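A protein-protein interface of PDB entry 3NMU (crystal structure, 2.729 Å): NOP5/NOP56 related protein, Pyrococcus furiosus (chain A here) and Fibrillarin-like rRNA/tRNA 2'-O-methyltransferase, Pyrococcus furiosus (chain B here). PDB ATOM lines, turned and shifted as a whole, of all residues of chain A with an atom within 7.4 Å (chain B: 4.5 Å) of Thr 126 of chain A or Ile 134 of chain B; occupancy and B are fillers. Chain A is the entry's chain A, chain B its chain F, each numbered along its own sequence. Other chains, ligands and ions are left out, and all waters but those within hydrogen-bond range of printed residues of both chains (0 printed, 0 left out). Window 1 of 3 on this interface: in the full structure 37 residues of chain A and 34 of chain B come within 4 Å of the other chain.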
ATOM      1  N   GLU A  42       2.978   6.465 -26.270  1.00  0.00           N
ATOM      2  CA  GLU A  42       4.176   5.698 -25.922  1.00  0.00           C
ATOM      3  C   GLU A  42       3.951   4.643 -24.838  1.00  0.00           C
ATOM      4  O   GLU A  42       4.671   3.645 -24.798  1.00  0.00           O
ATOM      5  CB  GLU A  42       5.346   6.607 -25.530  1.00  0.00           C
ATOM      6  CG  GLU A  42       5.198   7.365 -24.239  1.00  0.00           C
ATOM      7  CD  GLU A  42       4.602   8.740 -24.461  1.00  0.00           C
ATOM      8  OE1 GLU A  42       3.948   8.903 -25.520  1.00  0.00           O
ATOM      9  OE2 GLU A  42       4.792   9.645 -23.596  1.00  0.00           O
ATOM     10  N   LEU A  49       4.411  -3.510 -28.128  1.00  0.00           N
ATOM     11  CA  LEU A  49       5.590  -3.961 -28.868  1.00  0.00           C
ATOM     12  C   LEU A  49       6.247  -5.170 -28.207  1.00  0.00           C
ATOM     13  O   LEU A  49       6.645  -6.098 -28.903  1.00  0.00           O
ATOM     14  CB  LEU A  49       6.619  -2.837 -29.071  1.00  0.00           C
ATOM     15  CG  LEU A  49       6.291  -1.528 -29.812  1.00  0.00           C
ATOM     16  CD1 LEU A  49       7.338  -0.513 -29.465  1.00  0.00           C
ATOM     17  CD2 LEU A  49       6.188  -1.673 -31.321  1.00  0.00           C
ATOM     18  N   TYR A 118       5.632  10.227 -36.094  1.00  0.00           N
ATOM     19  CA  TYR A 118       6.482   9.074 -35.825  1.00  0.00           C
ATOM     20  C   TYR A 118       7.690   9.527 -34.997  1.00  0.00           C
ATOM     21  O   TYR A 118       8.313   8.733 -34.281  1.00  0.00           O
ATOM     22  CB  TYR A 118       6.944   8.437 -37.132  1.00  0.00           C
ATOM     23  CG  TYR A 118       6.097   7.282 -37.612  1.00  0.00           C
ATOM     24  CD1 TYR A 118       6.375   5.980 -37.205  1.00  0.00           C
ATOM     25  CD2 TYR A 118       5.039   7.485 -38.485  1.00  0.00           C
ATOM     26  CE1 TYR A 118       5.617   4.923 -37.629  1.00  0.00           C
ATOM     27  CE2 TYR A 118       4.270   6.431 -38.918  1.00  0.00           C
ATOM     28  CZ  TYR A 118       4.562   5.149 -38.486  1.00  0.00           C
ATOM     29  OH  TYR A 118       3.800   4.082 -38.923  1.00  0.00           O
ATOM     30  N   LYS A 120       7.518  12.425 -32.633  1.00  0.00           N
ATOM     31  CA  LYS A 120       7.154  12.804 -31.270  1.00  0.00           C
ATOM     32  C   LYS A 120       7.039  11.565 -30.400  1.00  0.00           C
ATOM     33  O   LYS A 120       7.646  11.481 -29.337  1.00  0.00           O
ATOM     34  CB  LYS A 120       5.868  13.642 -31.182  1.00  0.00           C
ATOM     35  CG  LYS A 120       5.677  14.245 -29.772  1.00  0.00           C
ATOM     36  CD  LYS A 120       4.326  14.929 -29.538  1.00  0.00           C
ATOM     37  CE  LYS A 120       3.208  13.937 -29.129  1.00  0.00           C
ATOM     38  NZ  LYS A 120       3.347  13.262 -27.788  1.00  0.00           N
ATOM     39  N   VAL A 121       6.272  10.592 -30.852  1.00  0.00           N
ATOM     40  CA  VAL A 121       6.159   9.362 -30.089  1.00  0.00           C
ATOM     41  C   VAL A 121       7.495   8.622 -29.964  1.00  0.00           C
ATOM     42  O   VAL A 121       7.859   8.176 -28.876  1.00  0.00           O
ATOM     43  CB  VAL A 121       5.136   8.400 -30.703  1.00  0.00           C
ATOM     44  CG1 VAL A 121       5.054   7.143 -29.870  1.00  0.00           C
ATOM     45  CG2 VAL A 121       3.781   9.072 -30.820  1.00  0.00           C
ATOM     46  N   GLY A 122       8.214   8.480 -31.078  1.00  0.00           N
ATOM     47  CA  GLY A 122       9.427   7.680 -31.107  1.00  0.00           C
ATOM     48  C   GLY A 122      10.427   8.079 -30.042  1.00  0.00           C
ATOM     49  O   GLY A 122      10.972   7.244 -29.326  1.00  0.00           O
ATOM     50  N   VAL A 123      10.682   9.373 -29.952  1.00  0.00           N
ATOM     51  CA  VAL A 123      11.600   9.876 -28.955  1.00  0.00           C
ATOM     52  C   VAL A 123      10.929   9.861 -27.574  1.00  0.00           C
ATOM     53  O   VAL A 123      11.597   9.706 -26.548  1.00  0.00           O
ATOM     54  CB  VAL A 123      12.156  11.276 -29.357  1.00  0.00           C
ATOM     55  CG1 VAL A 123      11.123  12.062 -30.137  1.00  0.00           C
ATOM     56  CG2 VAL A 123      12.646  12.062 -28.146  1.00  0.00           C
ATOM     57  N   ALA A 124       9.604   9.995 -27.549  1.00  0.00           N
ATOM     58  CA  ALA A 124       8.862   9.926 -26.284  1.00  0.00           C
ATOM     59  C   ALA A 124       8.964   8.537 -25.635  1.00  0.00           C
ATOM     60  O   ALA A 124       9.229   8.434 -24.441  1.00  0.00           O
ATOM     61  CB  ALA A 124       7.402  10.341 -26.468  1.00  0.00           C
ATOM     62  N   LEU A 125       8.776   7.478 -26.420  1.00  0.00           N
ATOM     63  CA  LEU A 125       8.943   6.117 -25.916  1.00  0.00           C
ATOM     64  C   LEU A 125      10.379   5.885 -25.480  1.00  0.00           C
ATOM     65  O   LEU A 125      10.653   5.056 -24.612  1.00  0.00           O
ATOM     66  CB  LEU A 125       8.534   5.077 -26.977  1.00  0.00           C
ATOM     67  CG  LEU A 125       9.031   3.624 -26.821  1.00  0.00           C
ATOM     68  CD1 LEU A 125       8.696   2.985 -25.486  1.00  0.00           C
ATOM     69  CD2 LEU A 125       8.517   2.734 -27.954  1.00  0.00           C
ATOM     70  N   THR A 126      11.304   6.612 -26.096  1.00  0.00           N
ATOM     71  CA  THR A 126      12.702   6.344 -25.841  1.00  0.00           C
ATOM     72  C   THR A 126      13.123   6.939 -24.519  1.00  0.00           C
ATOM     73  O   THR A 126      13.763   6.268 -23.713  1.00  0.00           O
ATOM     74  CB  THR A 126      13.592   6.827 -26.975  1.00  0.00           C
ATOM     75  OG1 THR A 126      13.246   6.106 -28.163  1.00  0.00           O
ATOM     76  CG2 THR A 126      15.055   6.569 -26.642  1.00  0.00           C
ATOM     77  N   ARG A 127      12.734   8.192 -24.292  1.00  0.00           N
ATOM     78  CA  ARG A 127      13.074   8.917 -23.066  1.00  0.00           C
ATOM     79  C   ARG A 127      12.315   8.334 -21.866  1.00  0.00           C
ATOM     80  O   ARG A 127      12.672   8.552 -20.694  1.00  0.00           O
ATOM     81  CB  ARG A 127      12.747  10.397 -23.231  1.00  0.00           C
ATOM     82  CG  ARG A 127      13.475  11.291 -22.256  1.00  0.00           C
ATOM     83  CD  ARG A 127      13.081  12.736 -22.476  1.00  0.00           C
ATOM     84  NE  ARG A 127      12.994  13.108 -23.896  1.00  0.00           N
ATOM     85  CZ  ARG A 127      13.903  13.836 -24.548  1.00  0.00           C
ATOM     86  NH1 ARG A 127      15.004  14.267 -23.932  1.00  0.00           N
ATOM     87  NH2 ARG A 127      13.711  14.137 -25.826  1.00  0.00           N
ATOM     88  N   MET A 128      11.256   7.597 -22.183  1.00  0.00           N
ATOM     89  CA  MET A 128      10.538   6.811 -21.203  1.00  0.00           C
ATOM     90  C   MET A 128      11.230   5.475 -20.911  1.00  0.00           C
ATOM     91  O   MET A 128      11.250   5.037 -19.770  1.00  0.00           O
ATOM     92  CB  MET A 128       9.094   6.610 -21.656  1.00  0.00           C
ATOM     93  CG  MET A 128       8.427   5.396 -21.090  1.00  0.00           C
ATOM     94  SD  MET A 128       6.763   5.152 -21.759  1.00  0.00           S
ATOM     95  CE  MET A 128       6.434   3.488 -21.166  1.00  0.00           C
ATOM     96  N   ARG A 129      11.804   4.833 -21.928  1.00  0.00           N
ATOM     97  CA  ARG A 129      12.502   3.559 -21.722  1.00  0.00           C
ATOM     98  C   ARG A 129      13.893   3.750 -21.083  1.00  0.00           C
ATOM     99  O   ARG A 129      14.463   2.800 -20.549  1.00  0.00           O
ATOM    100  CB  ARG A 129      12.668   2.793 -23.043  1.00  0.00           C
ATOM    101  CG  ARG A 129      11.409   2.410 -23.796  1.00  0.00           C
ATOM    102  CD  ARG A 129      11.621   1.044 -24.377  1.00  0.00           C
ATOM    103  NE  ARG A 129      10.421   0.399 -24.903  1.00  0.00           N
ATOM    104  CZ  ARG A 129      10.220   0.094 -26.188  1.00  0.00           C
ATOM    105  NH1 ARG A 129       9.102  -0.510 -26.561  1.00  0.00           N
ATOM    106  NH2 ARG A 129      11.128   0.394 -27.110  1.00  0.00           N
ATOM    107  N   ILE A 130      14.441   4.964 -21.150  1.00  0.00           N
ATOM    108  CA  ILE A 130      15.821   5.221 -20.703  1.00  0.00           C
ATOM    109  C   ILE A 130      15.926   5.971 -19.362  1.00  0.00           C
ATOM    110  O   ILE A 130      15.230   6.964 -19.121  1.00  0.00           O
ATOM    111  CB  ILE A 130      16.665   6.038 -21.762  1.00  0.00           C
ATOM    112  CG1 ILE A 130      16.561   5.441 -23.165  1.00  0.00           C
ATOM    113  CG2 ILE A 130      18.129   6.115 -21.355  1.00  0.00           C
ATOM    114  CD1 ILE A 130      17.550   6.037 -24.153  1.00  0.00           C
ATOM    115  N   GLN A 131      16.837   5.497 -18.516  1.00  0.00           N
ATOM    116  CA  GLN A 131      17.108   6.108 -17.218  1.00  0.00           C
ATOM    117  C   GLN A 131      17.852   7.419 -17.395  1.00  0.00           C
ATOM    118  O   GLN A 131      18.766   7.494 -18.206  1.00  0.00           O
ATOM    119  CB  GLN A 131      17.971   5.174 -16.366  1.00  0.00           C
ATOM    120  CG  GLN A 131      17.520   3.695 -16.338  1.00  0.00           C
ATOM    121  CD  GLN A 131      17.019   3.282 -14.972  1.00  0.00           C
ATOM    122  OE1 GLN A 131      16.086   3.883 -14.451  1.00  0.00           O
ATOM    123  NE2 GLN A 131      17.653   2.272 -14.372  1.00  0.00           N
ATOM    124  N   GLY B 110      16.999   5.460 -36.012  1.00  0.00           N
ATOM    125  CA  GLY B 110      18.157   4.853 -35.391  1.00  0.00           C
ATOM    126  C   GLY B 110      17.665   3.762 -34.480  1.00  0.00           C
ATOM    127  O   GLY B 110      16.684   3.978 -33.776  1.00  0.00           O
ATOM    128  N   ILE B 111      18.363   2.635 -34.429  1.00  0.00           N
ATOM    129  CA  ILE B 111      17.980   1.555 -33.531  1.00  0.00           C
ATOM    130  C   ILE B 111      19.210   1.162 -32.743  1.00  0.00           C
ATOM    131  O   ILE B 111      20.174   0.689 -33.307  1.00  0.00           O
ATOM    132  CB  ILE B 111      17.451   0.333 -34.322  1.00  0.00           C
ATOM    133  CG1 ILE B 111      15.928   0.234 -34.252  1.00  0.00           C
ATOM    134  CG2 ILE B 111      18.043  -0.954 -33.800  1.00  0.00           C
ATOM    135  CD1 ILE B 111      15.213   0.970 -35.345  1.00  0.00           C
ATOM    136  N   GLU B 112      19.202   1.372 -31.441  1.00  0.00           N
ATOM    137  CA  GLU B 112      20.410   1.119 -30.656  1.00  0.00           C
ATOM    138  C   GLU B 112      20.099   0.354 -29.398  1.00  0.00           C
ATOM    139  O   GLU B 112      19.302   0.779 -28.597  1.00  0.00           O
ATOM    140  CB  GLU B 112      21.127   2.423 -30.308  1.00  0.00           C
ATOM    141  CG  GLU B 112      22.155   2.318 -29.185  1.00  0.00           C
ATOM    142  CD  GLU B 112      23.292   1.355 -29.466  1.00  0.00           C
ATOM    143  OE1 GLU B 112      24.025   1.542 -30.456  1.00  0.00           O
ATOM    144  OE2 GLU B 112      23.479   0.413 -28.685  1.00  0.00           O
ATOM    145  N   LEU B 118      22.698   5.086 -26.458  1.00  0.00           N
ATOM    146  CA  LEU B 118      21.702   5.825 -27.232  1.00  0.00           C
ATOM    147  C   LEU B 118      21.407   7.167 -26.565  1.00  0.00           C
ATOM    148  O   LEU B 118      21.108   8.148 -27.237  1.00  0.00           O
ATOM    149  CB  LEU B 118      20.398   5.039 -27.433  1.00  0.00           C
ATOM    150  CG  LEU B 118      19.235   5.739 -28.162  1.00  0.00           C
ATOM    151  CD1 LEU B 118      19.630   6.247 -29.498  1.00  0.00           C
ATOM    152  CD2 LEU B 118      18.089   4.805 -28.357  1.00  0.00           C
ATOM    153  N   ILE B 132      15.085   9.662 -35.480  1.00  0.00           N
ATOM    154  CA  ILE B 132      14.321   9.175 -34.349  1.00  0.00           C
ATOM    155  C   ILE B 132      15.221   8.207 -33.608  1.00  0.00           C
ATOM    156  O   ILE B 132      15.618   7.198 -34.162  1.00  0.00           O
ATOM    157  CB  ILE B 132      13.048   8.470 -34.795  1.00  0.00           C
ATOM    158  CG1 ILE B 132      12.224   9.386 -35.695  1.00  0.00           C
ATOM    159  CG2 ILE B 132      12.231   8.073 -33.600  1.00  0.00           C
ATOM    160  CD1 ILE B 132      11.041   8.718 -36.327  1.00  0.00           C
ATOM    161  N   PRO B 133      15.637   8.556 -32.381  1.00  0.00           N
ATOM    162  CA  PRO B 133      16.393   7.557 -31.625  1.00  0.00           C
ATOM    163  C   PRO B 133      15.434   6.507 -31.125  1.00  0.00           C
ATOM    164  O   PRO B 133      14.462   6.868 -30.466  1.00  0.00           O
ATOM    165  CB  PRO B 133      16.925   8.336 -30.433  1.00  0.00           C
ATOM    166  CG  PRO B 133      16.218   9.684 -30.466  1.00  0.00           C
ATOM    167  CD  PRO B 133      15.174   9.649 -31.519  1.00  0.00           C
ATOM    168  N   ILE B 134      15.723   5.235 -31.353  1.00  0.00           N
ATOM    169  CA  ILE B 134      14.788   4.208 -30.956  1.00  0.00           C
ATOM    170  C   ILE B 134      15.528   3.157 -30.163  1.00  0.00           C
ATOM    171  O   ILE B 134      16.347   2.459 -30.713  1.00  0.00           O
ATOM    172  CB  ILE B 134      14.172   3.598 -32.219  1.00  0.00           C
ATOM    173  CG1 ILE B 134      13.133   4.556 -32.796  1.00  0.00           C
ATOM    174  CG2 ILE B 134      13.618   2.235 -31.958  1.00  0.00           C
ATOM    175  CD1 ILE B 134      12.316   3.975 -33.878  1.00  0.00           C
ATOM    176  N   LEU B 135      15.266   3.017 -28.871  1.00  0.00           N
ATOM    177  CA  LEU B 135      15.910   1.918 -28.162  1.00  0.00           C
ATOM    178  C   LEU B 135      15.304   0.585 -28.627  1.00  0.00           C
ATOM    179  O   LEU B 135      14.086   0.408 -28.660  1.00  0.00           O
ATOM    180  CB  LEU B 135      15.830   2.101 -26.653  1.00  0.00           C
ATOM    181  CG  LEU B 135      16.492   1.022 -25.789  1.00  0.00           C
ATOM    182  CD1 LEU B 135      17.984   1.222 -25.656  1.00  0.00           C
ATOM    183  CD2 LEU B 135      15.856   0.993 -24.381  1.00  0.00           C
ATOM    184  N   GLY B 136      16.159  -0.344 -29.020  1.00  0.00           N
ATOM    185  CA  GLY B 136      15.686  -1.593 -29.576  1.00  0.00           C
ATOM    186  C   GLY B 136      16.797  -2.599 -29.816  1.00  0.00           C
ATOM    187  O   GLY B 136      17.972  -2.293 -29.624  1.00  0.00           O
ATOM    188  N   TYR B 144      10.349  -3.190 -32.726  1.00  0.00           N
ATOM    189  CA  TYR B 144      10.184  -1.787 -33.196  1.00  0.00           C
ATOM    190  C   TYR B 144       9.134  -1.498 -34.275  1.00  0.00           C
ATOM    191  O   TYR B 144       9.161  -0.444 -34.920  1.00  0.00           O
ATOM    192  CB  TYR B 144      11.487  -1.020 -33.421  1.00  0.00           C
ATOM    193  CG  TYR B 144      12.594  -1.813 -34.024  1.00  0.00           C
ATOM    194  CD1 TYR B 144      12.836  -1.771 -35.380  1.00  0.00           C
ATOM    195  CD2 TYR B 144      13.428  -2.584 -33.232  1.00  0.00           C
ATOM    196  CE1 TYR B 144      13.869  -2.484 -35.931  1.00  0.00           C
ATOM    197  CE2 TYR B 144      14.469  -3.303 -33.778  1.00  0.00           C
ATOM    198  CZ  TYR B 144      14.687  -3.248 -35.126  1.00  0.00           C
ATOM    199  OH  TYR B 144      15.721  -3.975 -35.679  1.00  0.00           O
ATOM    200  N   LEU B 147       7.238   1.668 -34.594  1.00  0.00           N
ATOM    201  CA  LEU B 147       8.093   2.851 -34.490  1.00  0.00           C
ATOM    202  C   LEU B 147       8.561   3.345 -35.863  1.00  0.00           C
ATOM    203  O   LEU B 147       8.697   4.546 -36.073  1.00  0.00           O
ATOM    204  CB  LEU B 147       9.276   2.594 -33.542  1.00  0.00           C
ATOM    205  CG  LEU B 147       8.796   2.262 -32.128  1.00  0.00           C
ATOM    206  CD1 LEU B 147       9.900   2.331 -31.084  1.00  0.00           C
ATOM    207  CD2 LEU B 147       7.692   3.229 -31.785  1.00  0.00           C
ATOM    208  N   VAL B 148       8.748   2.408 -36.795  1.00  0.00           N
ATOM    209  CA  VAL B 148       9.386   2.684 -38.079  1.00  0.00           C
ATOM    210  C   VAL B 148       8.426   2.573 -39.270  1.00  0.00           C
ATOM    211  O   VAL B 148       7.252   2.334 -39.087  1.00  0.00           O
ATOM    212  CB  VAL B 148      10.587   1.740 -38.306  1.00  0.00           C
ATOM    213  CG1 VAL B 148      11.386   1.572 -37.018  1.00  0.00           C
ATOM    214  CG2 VAL B 148      10.110   0.412 -38.777  1.00  0.00           C
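The backbone carbonyl oxygen of Gly 122 of chain A lies within hydrogen-bond range of the side-chain hydroxyl of Thr 126 of chain A (2.8 Å). N of Gly 110 of chain B sits at hydrogen-bond distance from O of Ile 132 of chain B, at 2.9 Å. The backbone carbonyl oxygen (O) of Gly 110 of chain B is in hydrogen-bond range of the backbone NH (N) of Ile 134 of chain B, at 2.9 Å. O of Ile 134 of chain B is in hydrogen-bond range of N of Glu 112 of chain B.
Among the printed residues, merely in contact across the chains: Tyr 118 of chain A with Ile 132 of chain B (3.4 Å), Tyr 118 of chain A with Leu 147 of chain B (3.0 Å), Tyr 118 of chain A with Val 148 of chain B (3.4 Å), Gly 122 of chain A with Ile 132 of chain B (3.8 Å), Gly 122 of chain A with Pro 133 of chain B (3.7 Å), Leu 125 of chain A with Leu 147 of chain B (3.4 Å), Thr 126 of chain A with Leu 118 of chain B (3.9 Å), Thr 126 of chain A with Ile 134 of chain B (3.7 Å) and Thr 126 of chain A with Leu 135 of chain B (3.8 Å).
The backbone carbonyl oxygen of Pro 133 of chain B lies within hydrogen-bond range of the side-chain hydroxyl of Thr 126 of chain A. The guanidinium group of Arg 129 of chain A lies within hydrogen-bond range of the backbone carbonyl oxygen of Leu 135 of chain B, 3.3 Å away.
Of the 12 printed residues of chain B, 7 touch a printed residue of chain A. Hydrophobic or aromatic side chains of chain B within 4 Å of the printed part of chain A: Leu 118, Ile 132, Leu 135 and Leu 147. Printed residues of chain A that touch a printed residue of chain B: Tyr 118, Gly 122, Leu 125, Thr 126 and Arg 129. Among the printed residues, 11 pairs touch across the chains. Among the printed residues, no Asp or Glu carboxylate lies within 4 Å of a Lys or Arg side-chain nitrogen of the other chain.
Thr 126 of chain A touches just these residues of chain B: Leu 118, Pro 133, Ile 134 and Leu 135. Of chain A, only Thr 126 comes within 4 Å of Ile 134 of chain B. Of the printed residues of chain B, Tyr 118 of chain A touches Ile 132 (3.4 Å), Leu 147 (3.0 Å) and Val 148 (3.4 Å). Of the printed residues of chain A, Val 148 of chain B touches Tyr 118 (3.4 Å). Glu 112 of chain B touches none of the printed residues of chain A. The nearest printed residue of chain B that does not touch Gly 122 of chain A is Leu 147 of chain B (4.8 Å).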
